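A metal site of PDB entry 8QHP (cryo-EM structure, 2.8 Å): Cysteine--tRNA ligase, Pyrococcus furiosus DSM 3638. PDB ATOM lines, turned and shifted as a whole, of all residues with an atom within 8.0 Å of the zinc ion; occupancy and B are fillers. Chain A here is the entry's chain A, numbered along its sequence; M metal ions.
The side-chain sulfur (SG) of Cys 221 lies close to the side-chain amide nitrogen (ND2) of Asn 79. A ring nitrogen (ND1) of His 246 lies within hydrogen-bond range of a ring nitrogen (ND1) of His 218 (3.5 Å). N of Cys 41 sits at hydrogen-bond distance from O of Gly 237 (3.2 Å). The side-chain sulfur of Cys 41 sits close to a ring nitrogen (NE2) of His 247. O of Cys 221 lies close to OH of Tyr 39, 3.3 Å away. A ring nitrogen (NE2) of His 236 sits at hydrogen-bond distance from the side-chain carboxylate of Glu 250 (2.6 Å).
The zinc ion is bound by OE2 of Glu 250 (2.3 Å), SG of Cys 221 (2.3 Å), SG of Cys 41 (2.3 Å) and NE2 of His 246 (2.3 Å).
Of the 21 residues printed, 4 come within 4 Å of the zinc ion.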
ATOM      1  N   TYR A  39      -6.437 -33.120 -31.684  1.00  0.00           N
ATOM      2  CA  TYR A  39      -5.595 -32.771 -30.545  1.00  0.00           C
ATOM      3  C   TYR A  39      -5.751 -31.281 -30.266  1.00  0.00           C
ATOM      4  O   TYR A  39      -5.643 -30.465 -31.184  1.00  0.00           O
ATOM      5  CB  TYR A  39      -4.138 -33.118 -30.825  1.00  0.00           C
ATOM      6  CG  TYR A  39      -3.219 -32.896 -29.647  1.00  0.00           C
ATOM      7  CD1 TYR A  39      -2.983 -33.906 -28.730  1.00  0.00           C
ATOM      8  CD2 TYR A  39      -2.574 -31.677 -29.466  1.00  0.00           C
ATOM      9  CE1 TYR A  39      -2.145 -33.708 -27.660  1.00  0.00           C
ATOM     10  CE2 TYR A  39      -1.728 -31.476 -28.392  1.00  0.00           C
ATOM     11  CZ  TYR A  39      -1.517 -32.490 -27.494  1.00  0.00           C
ATOM     12  OH  TYR A  39      -0.674 -32.300 -26.429  1.00  0.00           O
ATOM     13  N   VAL A  40      -6.005 -30.932 -29.017  1.00  0.00           N
ATOM     14  CA  VAL A  40      -6.110 -29.529 -28.620  1.00  0.00           C
ATOM     15  C   VAL A  40      -5.120 -29.276 -27.497  1.00  0.00           C
ATOM     16  O   VAL A  40      -4.863 -30.138 -26.653  1.00  0.00           O
ATOM     17  CB  VAL A  40      -7.539 -29.145 -28.204  1.00  0.00           C
ATOM     18  CG1 VAL A  40      -8.525 -29.435 -29.330  1.00  0.00           C
ATOM     19  CG2 VAL A  40      -7.963 -29.872 -26.942  1.00  0.00           C
ATOM     20  N   CYS A  41      -4.546 -28.074 -27.506  1.00  0.00           N
ATOM     21  CA  CYS A  41      -3.611 -27.681 -26.460  1.00  0.00           C
ATOM     22  C   CYS A  41      -4.375 -27.312 -25.205  1.00  0.00           C
ATOM     23  O   CYS A  41      -5.208 -26.392 -25.229  1.00  0.00           O
ATOM     24  CB  CYS A  41      -2.737 -26.514 -26.927  1.00  0.00           C
ATOM     25  SG  CYS A  41      -1.482 -26.959 -28.146  1.00  0.00           S
ATOM     26  N   GLY A  42      -4.105 -28.011 -24.115  1.00  0.00           N
ATOM     27  CA  GLY A  42      -4.786 -27.762 -22.865  1.00  0.00           C
ATOM     28  C   GLY A  42      -4.247 -26.537 -22.170  1.00  0.00           C
ATOM     29  O   GLY A  42      -3.257 -25.919 -22.578  1.00  0.00           O
ATOM     30  N   ASN A  79      -3.865 -32.125 -23.744  1.00  0.00           N
ATOM     31  CA  ASN A  79      -2.785 -32.243 -22.784  1.00  0.00           C
ATOM     32  C   ASN A  79      -3.081 -31.443 -21.519  1.00  0.00           C
ATOM     33  O   ASN A  79      -3.914 -30.532 -21.512  1.00  0.00           O
ATOM     34  CB  ASN A  79      -1.465 -31.779 -23.406  1.00  0.00           C
ATOM     35  CG  ASN A  79      -1.574 -30.433 -24.092  1.00  0.00           C
ATOM     36  OD1 ASN A  79      -2.290 -29.545 -23.625  1.00  0.00           O
ATOM     37  ND2 ASN A  79      -0.862 -30.272 -25.195  1.00  0.00           N
ATOM     38  N   THR A  81      -0.648 -29.591 -19.084  1.00  0.00           N
ATOM     39  CA  THR A  81       0.676 -29.134 -18.674  1.00  0.00           C
ATOM     40  C   THR A  81       0.656 -28.829 -17.182  1.00  0.00           C
ATOM     41  O   THR A  81       0.126 -27.787 -16.772  1.00  0.00           O
ATOM     42  CB  THR A  81       1.104 -27.916 -19.486  1.00  0.00           C
ATOM     43  OG1 THR A  81       1.137 -28.255 -20.874  1.00  0.00           O
ATOM     44  CG2 THR A  81       2.475 -27.455 -19.053  1.00  0.00           C
ATOM     45  N   TRP A 217       8.699 -25.876 -23.199  1.00  0.00           N
ATOM     46  CA  TRP A 217       7.285 -25.522 -23.253  1.00  0.00           C
ATOM     47  C   TRP A 217       6.621 -25.924 -24.561  1.00  0.00           C
ATOM     48  O   TRP A 217       5.431 -25.658 -24.729  1.00  0.00           O
ATOM     49  CB  TRP A 217       7.110 -24.005 -23.032  1.00  0.00           C
ATOM     50  CG  TRP A 217       8.051 -23.424 -22.030  1.00  0.00           C
ATOM     51  CD1 TRP A 217       8.343 -23.904 -20.790  1.00  0.00           C
ATOM     52  CD2 TRP A 217       8.819 -22.221 -22.189  1.00  0.00           C
ATOM     53  NE1 TRP A 217       9.246 -23.092 -20.162  1.00  0.00           N
ATOM     54  CE2 TRP A 217       9.565 -22.046 -20.997  1.00  0.00           C
ATOM     55  CE3 TRP A 217       8.966 -21.290 -23.215  1.00  0.00           C
ATOM     56  CZ2 TRP A 217      10.431 -20.981 -20.815  1.00  0.00           C
ATOM     57  CZ3 TRP A 217       9.826 -20.224 -23.021  1.00  0.00           C
ATOM     58  CH2 TRP A 217      10.548 -20.078 -21.829  1.00  0.00           C
ATOM     59  N   HIS A 218       7.355 -26.544 -25.481  1.00  0.00           N
ATOM     60  CA  HIS A 218       6.804 -26.919 -26.777  1.00  0.00           C
ATOM     61  C   HIS A 218       6.953 -28.392 -27.107  1.00  0.00           C
ATOM     62  O   HIS A 218       6.201 -28.892 -27.955  1.00  0.00           O
ATOM     63  CB  HIS A 218       7.460 -26.086 -27.896  1.00  0.00           C
ATOM     64  CG  HIS A 218       7.533 -24.626 -27.608  1.00  0.00           C
ATOM     65  ND1 HIS A 218       6.415 -23.815 -27.580  1.00  0.00           N
ATOM     66  CD2 HIS A 218       8.585 -23.818 -27.333  1.00  0.00           C
ATOM     67  CE1 HIS A 218       6.778 -22.575 -27.308  1.00  0.00           C
ATOM     68  NE2 HIS A 218       8.089 -22.544 -27.145  1.00  0.00           N
ATOM     69  N   ILE A 219       7.904 -29.085 -26.478  1.00  0.00           N
ATOM     70  CA  ILE A 219       8.128 -30.503 -26.792  1.00  0.00           C
ATOM     71  C   ILE A 219       6.999 -31.366 -26.251  1.00  0.00           C
ATOM     72  O   ILE A 219       6.700 -32.426 -26.821  1.00  0.00           O
ATOM     73  CB  ILE A 219       9.504 -30.923 -26.232  1.00  0.00           C
ATOM     74  CG1 ILE A 219       9.900 -32.305 -26.750  1.00  0.00           C
ATOM     75  CG2 ILE A 219       9.502 -30.901 -24.718  1.00  0.00           C
ATOM     76  CD1 ILE A 219      10.379 -32.282 -28.174  1.00  0.00           C
ATOM     77  N   GLU A 220       6.336 -30.925 -25.181  1.00  0.00           N
ATOM     78  CA  GLU A 220       5.364 -31.769 -24.487  1.00  0.00           C
ATOM     79  C   GLU A 220       4.181 -32.113 -25.389  1.00  0.00           C
ATOM     80  O   GLU A 220       3.779 -33.279 -25.481  1.00  0.00           O
ATOM     81  CB  GLU A 220       4.885 -31.068 -23.224  1.00  0.00           C
ATOM     82  CG  GLU A 220       5.987 -30.414 -22.409  1.00  0.00           C
ATOM     83  CD  GLU A 220       5.451 -29.397 -21.418  1.00  0.00           C
ATOM     84  OE1 GLU A 220       4.255 -29.069 -21.499  1.00  0.00           O
ATOM     85  OE2 GLU A 220       6.238 -28.925 -20.575  1.00  0.00           O
ATOM     86  N   CYS A 221       3.605 -31.105 -26.036  1.00  0.00           N
ATOM     87  CA  CYS A 221       2.416 -31.338 -26.840  1.00  0.00           C
ATOM     88  C   CYS A 221       2.719 -32.240 -28.030  1.00  0.00           C
ATOM     89  O   CYS A 221       1.941 -33.136 -28.348  1.00  0.00           O
ATOM     90  CB  CYS A 221       1.834 -30.007 -27.311  1.00  0.00           C
ATOM     91  SG  CYS A 221       1.348 -28.880 -25.983  1.00  0.00           S
ATOM     92  N   SER A 222       3.863 -32.023 -28.694  1.00  0.00           N
ATOM     93  CA  SER A 222       4.250 -32.882 -29.800  1.00  0.00           C
ATOM     94  C   SER A 222       4.472 -34.313 -29.344  1.00  0.00           C
ATOM     95  O   SER A 222       4.020 -35.265 -30.004  1.00  0.00           O
ATOM     96  CB  SER A 222       5.494 -32.333 -30.481  1.00  0.00           C
ATOM     97  OG  SER A 222       5.905 -33.170 -31.554  1.00  0.00           O
ATOM     98  N   HIS A 236      -5.220 -30.310 -35.239  1.00  0.00           N
ATOM     99  CA  HIS A 236      -4.537 -29.718 -34.086  1.00  0.00           C
ATOM    100  C   HIS A 236      -5.174 -28.367 -33.807  1.00  0.00           C
ATOM    101  O   HIS A 236      -5.330 -27.549 -34.709  1.00  0.00           O
ATOM    102  CB  HIS A 236      -3.039 -29.560 -34.347  1.00  0.00           C
ATOM    103  CG  HIS A 236      -2.233 -29.364 -33.103  1.00  0.00           C
ATOM    104  ND1 HIS A 236      -2.446 -28.318 -32.235  1.00  0.00           N
ATOM    105  CD2 HIS A 236      -1.210 -30.089 -32.578  1.00  0.00           C
ATOM    106  CE1 HIS A 236      -1.588 -28.399 -31.227  1.00  0.00           C
ATOM    107  NE2 HIS A 236      -0.834 -29.464 -31.418  1.00  0.00           N
ATOM    108  N   GLY A 237      -5.541 -28.137 -32.539  1.00  0.00           N
ATOM    109  CA  GLY A 237      -6.277 -26.948 -32.184  1.00  0.00           C
ATOM    110  C   GLY A 237      -5.615 -26.193 -31.046  1.00  0.00           C
ATOM    111  O   GLY A 237      -4.741 -26.706 -30.350  1.00  0.00           O
ATOM    112  N   GLY A 238      -6.066 -24.961 -30.873  1.00  0.00           N
ATOM    113  CA  GLY A 238      -5.556 -24.122 -29.806  1.00  0.00           C
ATOM    114  C   GLY A 238      -5.979 -22.690 -30.021  1.00  0.00           C
ATOM    115  O   GLY A 238      -6.730 -22.362 -30.934  1.00  0.00           O
ATOM    116  N   LEU A 242      -1.264 -19.177 -29.855  1.00  0.00           N
ATOM    117  CA  LEU A 242      -0.412 -20.351 -29.990  1.00  0.00           C
ATOM    118  C   LEU A 242       0.137 -20.529 -31.395  1.00  0.00           C
ATOM    119  O   LEU A 242       1.022 -21.361 -31.588  1.00  0.00           O
ATOM    120  CB  LEU A 242      -1.177 -21.611 -29.580  1.00  0.00           C
ATOM    121  CG  LEU A 242      -1.629 -21.626 -28.121  1.00  0.00           C
ATOM    122  CD1 LEU A 242      -2.391 -22.900 -27.811  1.00  0.00           C
ATOM    123  CD2 LEU A 242      -0.435 -21.462 -27.192  1.00  0.00           C
ATOM    124  N   HIS A 246       4.257 -21.281 -30.342  1.00  0.00           N
ATOM    125  CA  HIS A 246       3.972 -22.603 -29.784  1.00  0.00           C
ATOM    126  C   HIS A 246       3.740 -23.647 -30.881  1.00  0.00           C
ATOM    127  O   HIS A 246       4.455 -24.646 -30.962  1.00  0.00           O
ATOM    128  CB  HIS A 246       2.759 -22.509 -28.848  1.00  0.00           C
ATOM    129  CG  HIS A 246       2.632 -23.664 -27.905  1.00  0.00           C
ATOM    130  ND1 HIS A 246       3.100 -23.614 -26.607  1.00  0.00           N
ATOM    131  CD2 HIS A 246       2.097 -24.891 -28.064  1.00  0.00           C
ATOM    132  CE1 HIS A 246       2.853 -24.757 -26.005  1.00  0.00           C
ATOM    133  NE2 HIS A 246       2.246 -25.556 -26.862  1.00  0.00           N
ATOM    134  N   HIS A 247       2.735 -23.424 -31.735  1.00  0.00           N
ATOM    135  CA  HIS A 247       2.388 -24.440 -32.725  1.00  0.00           C
ATOM    136  C   HIS A 247       3.408 -24.511 -33.849  1.00  0.00           C
ATOM    137  O   HIS A 247       3.596 -25.596 -34.420  1.00  0.00           O
ATOM    138  CB  HIS A 247       0.992 -24.172 -33.266  1.00  0.00           C
ATOM    139  CG  HIS A 247      -0.100 -24.428 -32.268  1.00  0.00           C
ATOM    140  ND1 HIS A 247      -1.432 -24.430 -32.616  1.00  0.00           N
ATOM    141  CD2 HIS A 247      -0.053 -24.698 -30.950  1.00  0.00           C
ATOM    142  CE1 HIS A 247      -2.165 -24.686 -31.539  1.00  0.00           C
ATOM    143  NE2 HIS A 247      -1.346 -24.858 -30.520  1.00  0.00           N
ATOM    144  N   GLU A 250       5.840 -26.773 -32.448  1.00  0.00           N
ATOM    145  CA  GLU A 250       5.335 -28.143 -32.471  1.00  0.00           C
ATOM    146  C   GLU A 250       5.514 -28.776 -33.852  1.00  0.00           C
ATOM    147  O   GLU A 250       6.015 -29.892 -33.979  1.00  0.00           O
ATOM    148  CB  GLU A 250       3.859 -28.182 -32.075  1.00  0.00           C
ATOM    149  CG  GLU A 250       3.577 -27.800 -30.637  1.00  0.00           C
ATOM    150  CD  GLU A 250       2.182 -28.214 -30.204  1.00  0.00           C
ATOM    151  OE1 GLU A 250       1.691 -29.247 -30.703  1.00  0.00           O
ATOM    152  OE2 GLU A 250       1.581 -27.519 -29.360  1.00  0.00           O
ATOM    153  N   TRP A 262       2.748 -33.833 -40.368  1.00  0.00           N
ATOM    154  CA  TRP A 262       2.338 -34.191 -39.018  1.00  0.00           C
ATOM    155  C   TRP A 262       0.855 -33.932 -38.759  1.00  0.00           C
ATOM    156  O   TRP A 262       0.143 -34.831 -38.314  1.00  0.00           O
ATOM    157  CB  TRP A 262       3.188 -33.410 -38.012  1.00  0.00           C
ATOM    158  CG  TRP A 262       2.787 -33.606 -36.585  1.00  0.00           C
ATOM    159  CD1 TRP A 262       2.553 -34.791 -35.950  1.00  0.00           C
ATOM    160  CD2 TRP A 262       2.600 -32.574 -35.609  1.00  0.00           C
ATOM    161  NE1 TRP A 262       2.220 -34.555 -34.635  1.00  0.00           N
ATOM    162  CE2 TRP A 262       2.243 -33.203 -34.401  1.00  0.00           C
ATOM    163  CE3 TRP A 262       2.711 -31.179 -35.635  1.00  0.00           C
ATOM    164  CZ2 TRP A 262       1.989 -32.488 -33.235  1.00  0.00           C
ATOM    165  CZ3 TRP A 262       2.453 -30.475 -34.478  1.00  0.00           C
ATOM    166  CH2 TRP A 262       2.095 -31.132 -33.292  1.00  0.00           C
ATOM    167  N   TRP A 266      -5.061 -27.324 -39.308  1.00  0.00           N
ATOM    168  CA  TRP A 266      -4.791 -26.507 -38.127  1.00  0.00           C
ATOM    169  C   TRP A 266      -5.968 -25.571 -37.893  1.00  0.00           C
ATOM    170  O   TRP A 266      -6.346 -24.809 -38.796  1.00  0.00           O
ATOM    171  CB  TRP A 266      -3.503 -25.705 -38.296  1.00  0.00           C
ATOM    172  CG  TRP A 266      -2.266 -26.547 -38.280  1.00  0.00           C
ATOM    173  CD1 TRP A 266      -1.690 -27.168 -39.339  1.00  0.00           C
ATOM    174  CD2 TRP A 266      -1.452 -26.846 -37.143  1.00  0.00           C
ATOM    175  NE1 TRP A 266      -0.569 -27.848 -38.944  1.00  0.00           N
ATOM    176  CE2 TRP A 266      -0.398 -27.662 -37.595  1.00  0.00           C
ATOM    177  CE3 TRP A 266      -1.508 -26.499 -35.790  1.00  0.00           C
ATOM    178  CZ2 TRP A 266       0.587 -28.138 -36.738  1.00  0.00           C
ATOM    179  CZ3 TRP A 266      -0.526 -26.985 -34.942  1.00  0.00           C
ATOM    180  CH2 TRP A 266       0.499 -27.792 -35.416  1.00  0.00           C
HETATM  181 ZN    ZN M   1       0.661 -27.156 -27.338  1.00  0.00          ZN
